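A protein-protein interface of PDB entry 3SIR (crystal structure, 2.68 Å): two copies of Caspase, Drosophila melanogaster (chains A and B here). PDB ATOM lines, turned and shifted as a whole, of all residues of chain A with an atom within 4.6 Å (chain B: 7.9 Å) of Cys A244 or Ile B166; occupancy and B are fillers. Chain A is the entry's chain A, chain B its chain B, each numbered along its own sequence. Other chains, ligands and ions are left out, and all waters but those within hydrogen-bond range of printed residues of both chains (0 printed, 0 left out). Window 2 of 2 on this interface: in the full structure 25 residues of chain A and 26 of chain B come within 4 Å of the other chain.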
ATOM      1  N   LEU A 143     -23.761 -22.003 -18.605  1.00  0.00           N
ATOM      2  CA  LEU A 143     -22.986 -20.818 -18.949  1.00  0.00           C
ATOM      3  C   LEU A 143     -21.679 -21.177 -19.650  1.00  0.00           C
ATOM      4  O   LEU A 143     -20.885 -21.962 -19.135  1.00  0.00           O
ATOM      5  CB  LEU A 143     -22.703 -19.977 -17.705  1.00  0.00           C
ATOM      6  CG  LEU A 143     -21.907 -18.688 -17.924  1.00  0.00           C
ATOM      7  CD1 LEU A 143     -22.635 -17.743 -18.874  1.00  0.00           C
ATOM      8  CD2 LEU A 143     -21.642 -18.008 -16.587  1.00  0.00           C
ATOM      9  N   ASP A 144     -21.486 -20.631 -20.845  1.00  0.00           N
ATOM     10  CA  ASP A 144     -20.324 -20.963 -21.653  1.00  0.00           C
ATOM     11  C   ASP A 144     -19.842 -19.730 -22.408  1.00  0.00           C
ATOM     12  O   ASP A 144     -20.615 -18.801 -22.646  1.00  0.00           O
ATOM     13  CB  ASP A 144     -20.655 -22.087 -22.636  1.00  0.00           C
ATOM     14  CG  ASP A 144     -21.966 -22.780 -22.314  1.00  0.00           C
ATOM     15  OD1 ASP A 144     -21.951 -24.001 -22.051  1.00  0.00           O
ATOM     16  OD2 ASP A 144     -23.017 -22.107 -22.353  1.00  0.00           O
ATOM     17  N   ILE A 174     -20.895  -9.727 -16.799  1.00  0.00           N
ATOM     18  CA  ILE A 174     -22.014 -10.601 -16.471  1.00  0.00           C
ATOM     19  C   ILE A 174     -21.760 -11.337 -15.158  1.00  0.00           C
ATOM     20  O   ILE A 174     -21.019 -12.318 -15.128  1.00  0.00           O
ATOM     21  CB  ILE A 174     -22.258 -11.628 -17.599  1.00  0.00           C
ATOM     22  CG1 ILE A 174     -22.789 -10.928 -18.854  1.00  0.00           C
ATOM     23  CG2 ILE A 174     -23.242 -12.702 -17.148  1.00  0.00           C
ATOM     24  CD1 ILE A 174     -21.732 -10.649 -19.893  1.00  0.00           C
ATOM     25  N   ALA A 175     -22.329 -10.836 -14.063  1.00  0.00           N
ATOM     26  CA  ALA A 175     -22.426 -11.611 -12.826  1.00  0.00           C
ATOM     27  C   ALA A 175     -23.529 -12.665 -12.906  1.00  0.00           C
ATOM     28  O   ALA A 175     -24.673 -12.362 -13.246  1.00  0.00           O
ATOM     29  CB  ALA A 175     -22.657 -10.692 -11.641  1.00  0.00           C
ATOM     30  N   TYR A 176     -23.182 -13.911 -12.611  1.00  0.00           N
ATOM     31  CA  TYR A 176     -24.063 -15.028 -12.922  1.00  0.00           C
ATOM     32  C   TYR A 176     -24.086 -16.076 -11.812  1.00  0.00           C
ATOM     33  O   TYR A 176     -23.041 -16.546 -11.367  1.00  0.00           O
ATOM     34  CB  TYR A 176     -23.657 -15.674 -14.246  1.00  0.00           C
ATOM     35  CG  TYR A 176     -24.508 -16.861 -14.631  1.00  0.00           C
ATOM     36  CD1 TYR A 176     -25.398 -16.785 -15.696  1.00  0.00           C
ATOM     37  CD2 TYR A 176     -24.390 -18.071 -13.959  1.00  0.00           C
ATOM     38  CE1 TYR A 176     -26.162 -17.875 -16.064  1.00  0.00           C
ATOM     39  CE2 TYR A 176     -25.121 -19.178 -14.348  1.00  0.00           C
ATOM     40  CZ  TYR A 176     -26.022 -19.066 -15.383  1.00  0.00           C
ATOM     41  OH  TYR A 176     -26.824 -20.134 -15.705  1.00  0.00           O
ATOM     42  N   ILE A 242     -21.654 -20.821  -6.908  1.00  0.00           N
ATOM     43  CA  ILE A 242     -21.072 -19.592  -6.378  1.00  0.00           C
ATOM     44  C   ILE A 242     -21.021 -18.571  -7.508  1.00  0.00           C
ATOM     45  O   ILE A 242     -21.032 -18.944  -8.680  1.00  0.00           O
ATOM     46  CB  ILE A 242     -19.652 -19.832  -5.821  1.00  0.00           C
ATOM     47  CG1 ILE A 242     -19.028 -18.521  -5.335  1.00  0.00           C
ATOM     48  CG2 ILE A 242     -18.760 -20.484  -6.872  1.00  0.00           C
ATOM     49  CD1 ILE A 242     -17.512 -18.514  -5.389  1.00  0.00           C
ATOM     50  N   PRO A 243     -21.040 -17.274  -7.168  1.00  0.00           N
ATOM     51  CA  PRO A 243     -21.164 -16.331  -8.270  1.00  0.00           C
ATOM     52  C   PRO A 243     -19.996 -16.409  -9.251  1.00  0.00           C
ATOM     53  O   PRO A 243     -18.850 -16.631  -8.856  1.00  0.00           O
ATOM     54  CB  PRO A 243     -21.208 -14.978  -7.562  1.00  0.00           C
ATOM     55  CG  PRO A 243     -21.884 -15.285  -6.272  1.00  0.00           C
ATOM     56  CD  PRO A 243     -21.439 -16.674  -5.884  1.00  0.00           C
ATOM     57  N   CYS A 244     -20.327 -16.358 -10.535  1.00  0.00           N
ATOM     58  CA  CYS A 244     -19.347 -16.520 -11.594  1.00  0.00           C
ATOM     59  C   CYS A 244     -19.293 -15.236 -12.411  1.00  0.00           C
ATOM     60  O   CYS A 244     -20.162 -14.979 -13.249  1.00  0.00           O
ATOM     61  CB  CYS A 244     -19.734 -17.701 -12.485  1.00  0.00           C
ATOM     62  SG  CYS A 244     -19.309 -17.482 -14.225  1.00  0.00           S
ATOM     63  N   ILE A 245     -18.330 -14.378 -12.094  1.00  0.00           N
ATOM     64  CA  ILE A 245     -18.291 -13.061 -12.711  1.00  0.00           C
ATOM     65  C   ILE A 245     -17.389 -13.094 -13.933  1.00  0.00           C
ATOM     66  O   ILE A 245     -16.277 -13.617 -13.872  1.00  0.00           O
ATOM     67  CB  ILE A 245     -17.782 -11.996 -11.733  1.00  0.00           C
ATOM     68  CG1 ILE A 245     -18.800 -11.782 -10.610  1.00  0.00           C
ATOM     69  CG2 ILE A 245     -17.505 -10.696 -12.471  1.00  0.00           C
ATOM     70  CD1 ILE A 245     -18.187 -11.782  -9.228  1.00  0.00           C
ATOM     71  N   THR A 246     -17.875 -12.557 -15.046  1.00  0.00           N
ATOM     72  CA  THR A 246     -17.096 -12.547 -16.276  1.00  0.00           C
ATOM     73  C   THR A 246     -16.973 -11.139 -16.851  1.00  0.00           C
ATOM     74  O   THR A 246     -17.925 -10.608 -17.426  1.00  0.00           O
ATOM     75  CB  THR A 246     -17.710 -13.476 -17.338  1.00  0.00           C
ATOM     76  OG1 THR A 246     -17.704 -12.814 -18.608  1.00  0.00           O
ATOM     77  CG2 THR A 246     -19.142 -13.823 -16.973  1.00  0.00           C
ATOM     78  N   TRP B 115     -10.984 -29.650 -14.894  1.00  0.00           N
ATOM     79  CA  TRP B 115     -10.976 -28.764 -13.739  1.00  0.00           C
ATOM     80  C   TRP B 115     -11.034 -29.588 -12.461  1.00  0.00           C
ATOM     81  O   TRP B 115     -10.311 -29.307 -11.505  1.00  0.00           O
ATOM     82  CB  TRP B 115     -12.186 -27.832 -13.798  1.00  0.00           C
ATOM     83  CG  TRP B 115     -12.530 -27.415 -15.194  1.00  0.00           C
ATOM     84  CD1 TRP B 115     -12.870 -28.235 -16.236  1.00  0.00           C
ATOM     85  CD2 TRP B 115     -12.450 -26.089 -15.734  1.00  0.00           C
ATOM     86  NE1 TRP B 115     -13.027 -27.497 -17.385  1.00  0.00           N
ATOM     87  CE2 TRP B 115     -12.787 -26.176 -17.101  1.00  0.00           C
ATOM     88  CE3 TRP B 115     -12.134 -24.836 -15.192  1.00  0.00           C
ATOM     89  CZ2 TRP B 115     -12.811 -25.059 -17.934  1.00  0.00           C
ATOM     90  CZ3 TRP B 115     -12.187 -23.724 -16.014  1.00  0.00           C
ATOM     91  CH2 TRP B 115     -12.501 -23.846 -17.375  1.00  0.00           C
ATOM     92  N   TYR B 164     -16.321 -22.575 -25.265  1.00  0.00           N
ATOM     93  CA  TYR B 164     -16.068 -23.404 -24.089  1.00  0.00           C
ATOM     94  C   TYR B 164     -17.068 -23.166 -22.961  1.00  0.00           C
ATOM     95  O   TYR B 164     -17.554 -22.050 -22.771  1.00  0.00           O
ATOM     96  CB  TYR B 164     -14.645 -23.175 -23.581  1.00  0.00           C
ATOM     97  CG  TYR B 164     -14.534 -22.059 -22.570  1.00  0.00           C
ATOM     98  CD1 TYR B 164     -14.518 -22.330 -21.209  1.00  0.00           C
ATOM     99  CD2 TYR B 164     -14.435 -20.737 -22.978  1.00  0.00           C
ATOM    100  CE1 TYR B 164     -14.405 -21.314 -20.280  1.00  0.00           C
ATOM    101  CE2 TYR B 164     -14.318 -19.712 -22.055  1.00  0.00           C
ATOM    102  CZ  TYR B 164     -14.297 -20.007 -20.709  1.00  0.00           C
ATOM    103  OH  TYR B 164     -14.173 -18.991 -19.790  1.00  0.00           O
ATOM    104  N   LYS B 165     -17.273 -24.193 -22.142  1.00  0.00           N
ATOM    105  CA  LYS B 165     -18.193 -24.108 -21.016  1.00  0.00           C
ATOM    106  C   LYS B 165     -17.405 -23.881 -19.735  1.00  0.00           C
ATOM    107  O   LYS B 165     -16.278 -24.353 -19.610  1.00  0.00           O
ATOM    108  CB  LYS B 165     -18.995 -25.404 -20.885  1.00  0.00           C
ATOM    109  CG  LYS B 165     -18.577 -26.256 -19.691  1.00  0.00           C
ATOM    110  CD  LYS B 165     -19.573 -27.371 -19.398  1.00  0.00           C
ATOM    111  CE  LYS B 165     -20.559 -26.968 -18.311  1.00  0.00           C
ATOM    112  NZ  LYS B 165     -20.047 -27.267 -16.944  1.00  0.00           N
ATOM    113  N   ILE B 166     -18.056 -23.295 -18.735  1.00  0.00           N
ATOM    114  CA  ILE B 166     -17.494 -23.253 -17.390  1.00  0.00           C
ATOM    115  C   ILE B 166     -18.544 -23.226 -16.278  1.00  0.00           C
ATOM    116  O   ILE B 166     -19.650 -22.719 -16.471  1.00  0.00           O
ATOM    117  CB  ILE B 166     -16.551 -22.058 -17.221  1.00  0.00           C
ATOM    118  CG1 ILE B 166     -17.181 -20.799 -17.822  1.00  0.00           C
ATOM    119  CG2 ILE B 166     -15.198 -22.363 -17.846  1.00  0.00           C
ATOM    120  CD1 ILE B 166     -17.941 -19.961 -16.819  1.00  0.00           C
ATOM    121  N   PRO B 167     -18.242 -23.896 -15.155  1.00  0.00           N
ATOM    122  CA  PRO B 167     -18.625 -23.416 -13.835  1.00  0.00           C
ATOM    123  C   PRO B 167     -17.390 -23.201 -12.955  1.00  0.00           C
ATOM    124  O   PRO B 167     -16.559 -22.346 -13.265  1.00  0.00           O
ATOM    125  CB  PRO B 167     -19.483 -24.567 -13.300  1.00  0.00           C
ATOM    126  CG  PRO B 167     -18.997 -25.804 -14.035  1.00  0.00           C
ATOM    127  CD  PRO B 167     -18.095 -25.361 -15.163  1.00  0.00           C
ATOM    128  N   VAL B 168     -17.255 -23.979 -11.881  1.00  0.00           N
ATOM    129  CA  VAL B 168     -18.113 -23.872 -10.704  1.00  0.00           C
ATOM    130  C   VAL B 168     -17.375 -23.072  -9.636  1.00  0.00           C
ATOM    131  O   VAL B 168     -17.875 -22.059  -9.147  1.00  0.00           O
ATOM    132  CB  VAL B 168     -18.450 -25.263 -10.112  1.00  0.00           C
ATOM    133  CG1 VAL B 168     -18.768 -25.152  -8.626  1.00  0.00           C
ATOM    134  CG2 VAL B 168     -19.620 -25.908 -10.850  1.00  0.00           C
ATOM    135  N   HIS B 169     -16.132 -23.461  -9.373  1.00  0.00           N
ATOM    136  CA  HIS B 169     -15.638 -23.557  -8.007  1.00  0.00           C
ATOM    137  C   HIS B 169     -14.879 -22.306  -7.588  1.00  0.00           C
ATOM    138  O   HIS B 169     -14.420 -21.528  -8.423  1.00  0.00           O
ATOM    139  CB  HIS B 169     -14.753 -24.797  -7.849  1.00  0.00           C
ATOM    140  CG  HIS B 169     -15.108 -25.651  -6.670  1.00  0.00           C
ATOM    141  ND1 HIS B 169     -15.094 -25.180  -5.374  1.00  0.00           N
ATOM    142  CD2 HIS B 169     -15.414 -26.968  -6.584  1.00  0.00           C
ATOM    143  CE1 HIS B 169     -15.361 -26.170  -4.542  1.00  0.00           C
ATOM    144  NE2 HIS B 169     -15.534 -27.271  -5.249  1.00  0.00           N
ATOM    145  N   PHE B 172     -11.127 -19.908  -8.462  1.00  0.00           N
ATOM    146  CA  PHE B 172     -10.703 -20.092  -9.849  1.00  0.00           C
ATOM    147  C   PHE B 172     -10.727 -18.772 -10.614  1.00  0.00           C
ATOM    148  O   PHE B 172     -11.650 -17.973 -10.458  1.00  0.00           O
ATOM    149  CB  PHE B 172     -11.649 -21.065 -10.559  1.00  0.00           C
ATOM    150  CG  PHE B 172     -11.333 -22.516 -10.326  1.00  0.00           C
ATOM    151  CD1 PHE B 172     -11.151 -23.007  -9.046  1.00  0.00           C
ATOM    152  CD2 PHE B 172     -11.402 -23.419 -11.373  1.00  0.00           C
ATOM    153  CE1 PHE B 172     -10.944 -24.361  -8.826  1.00  0.00           C
ATOM    154  CE2 PHE B 172     -11.208 -24.775 -11.160  1.00  0.00           C
ATOM    155  CZ  PHE B 172     -10.975 -25.244  -9.886  1.00  0.00           C
ATOM    156  N   ILE B 174      -9.995 -17.445 -14.947  1.00  0.00           N
ATOM    157  CA  ILE B 174      -9.786 -17.964 -16.292  1.00  0.00           C
ATOM    158  C   ILE B 174      -9.712 -16.834 -17.310  1.00  0.00           C
ATOM    159  O   ILE B 174     -10.734 -16.329 -17.773  1.00  0.00           O
ATOM    160  CB  ILE B 174     -10.893 -18.955 -16.693  1.00  0.00           C
ATOM    161  CG1 ILE B 174     -10.654 -20.310 -16.023  1.00  0.00           C
ATOM    162  CG2 ILE B 174     -10.941 -19.109 -18.203  1.00  0.00           C
ATOM    163  CD1 ILE B 174     -11.468 -20.534 -14.766  1.00  0.00           C
ATOM    164  N   TYR B 176      -8.960 -15.678 -20.967  1.00  0.00           N
ATOM    165  CA  TYR B 176      -9.236 -16.431 -22.181  1.00  0.00           C
ATOM    166  C   TYR B 176      -9.303 -15.485 -23.376  1.00  0.00           C
ATOM    167  O   TYR B 176     -10.226 -14.678 -23.485  1.00  0.00           O
ATOM    168  CB  TYR B 176     -10.558 -17.189 -22.031  1.00  0.00           C
ATOM    169  CG  TYR B 176     -10.935 -18.020 -23.238  1.00  0.00           C
ATOM    170  CD1 TYR B 176     -10.756 -19.401 -23.241  1.00  0.00           C
ATOM    171  CD2 TYR B 176     -11.472 -17.428 -24.373  1.00  0.00           C
ATOM    172  CE1 TYR B 176     -11.103 -20.166 -24.336  1.00  0.00           C
ATOM    173  CE2 TYR B 176     -11.839 -18.189 -25.471  1.00  0.00           C
ATOM    174  CZ  TYR B 176     -11.632 -19.552 -25.453  1.00  0.00           C
ATOM    175  OH  TYR B 176     -11.971 -20.301 -26.556  1.00  0.00           O
ATOM    176  N   CYS B 244     -11.410 -12.323 -22.446  1.00  0.00           N
ATOM    177  CA  CYS B 244     -12.563 -12.535 -21.586  1.00  0.00           C
ATOM    178  C   CYS B 244     -12.080 -13.102 -20.264  1.00  0.00           C
ATOM    179  O   CYS B 244     -11.196 -13.959 -20.243  1.00  0.00           O
ATOM    180  CB  CYS B 244     -13.559 -13.485 -22.251  1.00  0.00           C
ATOM    181  SG  CYS B 244     -14.748 -14.209 -21.110  1.00  0.00           S
ATOM    182  N   ILE B 245     -12.506 -12.471 -19.175  1.00  0.00           N
ATOM    183  CA  ILE B 245     -11.986 -12.766 -17.844  1.00  0.00           C
ATOM    184  C   ILE B 245     -13.147 -13.099 -16.917  1.00  0.00           C
ATOM    185  O   ILE B 245     -14.120 -12.345 -16.811  1.00  0.00           O
ATOM    186  CB  ILE B 245     -11.246 -11.550 -17.246  1.00  0.00           C
ATOM    187  CG1 ILE B 245     -10.058 -11.141 -18.124  1.00  0.00           C
ATOM    188  CG2 ILE B 245     -10.811 -11.833 -15.808  1.00  0.00           C
ATOM    189  CD1 ILE B 245      -9.553  -9.722 -17.846  1.00  0.00           C
ATOM    190  N   THR B 246     -13.000 -14.188 -16.177  1.00  0.00           N
ATOM    191  CA  THR B 246     -14.110 -14.731 -15.413  1.00  0.00           C
ATOM    192  C   THR B 246     -13.567 -15.297 -14.109  1.00  0.00           C
ATOM    193  O   THR B 246     -12.634 -16.097 -14.122  1.00  0.00           O
ATOM    194  CB  THR B 246     -14.840 -15.822 -16.221  1.00  0.00           C
ATOM    195  OG1 THR B 246     -15.055 -16.972 -15.398  1.00  0.00           O
ATOM    196  CG2 THR B 246     -14.012 -16.230 -17.435  1.00  0.00           C
ATOM    197  N   THR B 247     -13.990 -14.711 -12.994  1.00  0.00           N
ATOM    198  CA  THR B 247     -13.283 -14.884 -11.734  1.00  0.00           C
ATOM    199  C   THR B 247     -14.237 -15.377 -10.656  1.00  0.00           C
ATOM    200  O   THR B 247     -15.375 -14.922 -10.587  1.00  0.00           O
ATOM    201  CB  THR B 247     -12.665 -13.564 -11.254  1.00  0.00           C
ATOM    202  OG1 THR B 247     -12.621 -13.555  -9.822  1.00  0.00           O
ATOM    203  CG2 THR B 247     -13.504 -12.389 -11.729  1.00  0.00           C
ATOM    204  N   MET B 248     -13.779 -16.322  -9.839  1.00  0.00           N
ATOM    205  CA  MET B 248     -14.475 -16.677  -8.609  1.00  0.00           C
ATOM    206  C   MET B 248     -13.653 -16.322  -7.377  1.00  0.00           C
ATOM    207  O   MET B 248     -14.051 -16.600  -6.246  1.00  0.00           O
ATOM    208  CB  MET B 248     -14.816 -18.165  -8.587  1.00  0.00           C
ATOM    209  CG  MET B 248     -16.179 -18.470  -9.162  1.00  0.00           C
ATOM    210  SD  MET B 248     -16.182 -18.219 -10.941  1.00  0.00           S
ATOM    211  CE  MET B 248     -16.764 -19.826 -11.481  1.00  0.00           C
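The backbone carbonyl oxygen (O) of Leu A143 sits at hydrogen-bond distance from the backbone NH (N) of Ile B166 (3.2 Å). O of Pro A243 lies close to SD of Met B248 (3.7 Å). O of Ile A245 lies within hydrogen-bond range of N of Thr B247 (2.7 Å).
Ile B245 touches its own counterpart, Ile A245. Ile A245 touches Thr B246, and with the chains exchanged Thr A246 touches Ile B245. Thr A246 touches its own counterpart, Thr B246. 5 positions are printed for both chains. Of the 14 pairs that touch across the chains among the printed residues, 4 have their exchanged pair printed and touching as well.
O of Leu A143 touches CA of Lys B165, 3.9 Å away. Asp A144 touches Tyr B164 (CB to O, 3.1 Å). Asp A144 touches Lys B165. Ile A242 touches Val B168. Met B248 touches Ile A242 (CG to CG2, 3.995 Å). Cys A244 touches Ile B166. Ile A245 touches Ile B245. Ile A245 touches Thr B246 (O to CA, 2.9 Å). Thr A246 touches Ile B245. Thr A246 touches Thr B246 (CA to CA, 3.8 Å).
Of chain B, only Ile B166 (3.8 Å) and Met B248 (3.7 Å) come within 4 Å of Cys A244. Ile B166 touches two residues of chain A. Printed residues of chain B within 4 Å of Ile A242: Val B168 (2.9 Å) and Met B248 (3.995 Å). Of the printed residues of chain A, Thr B247 touches Ile A245 (2.7 Å).
The backbone NH (N) of Cys A244 is in hydrogen-bond range of the backbone carbonyl oxygen (O) of Tyr A176, 2.8 Å away. O of Ile A174 sits close to N of Thr A246, at 3.2 Å. O of Phe B172 sits at hydrogen-bond distance from N of Met B248, at 2.8 Å. O of Thr B246 sits at hydrogen-bond distance from N of Ile B174, at 3.1 Å.
Of the 15 printed residues of chain B, 8 touch a printed residue of chain A. Hydrophobic or aromatic side chains of chain B that line the printed part of chain A: Ile B166 and Met B248.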
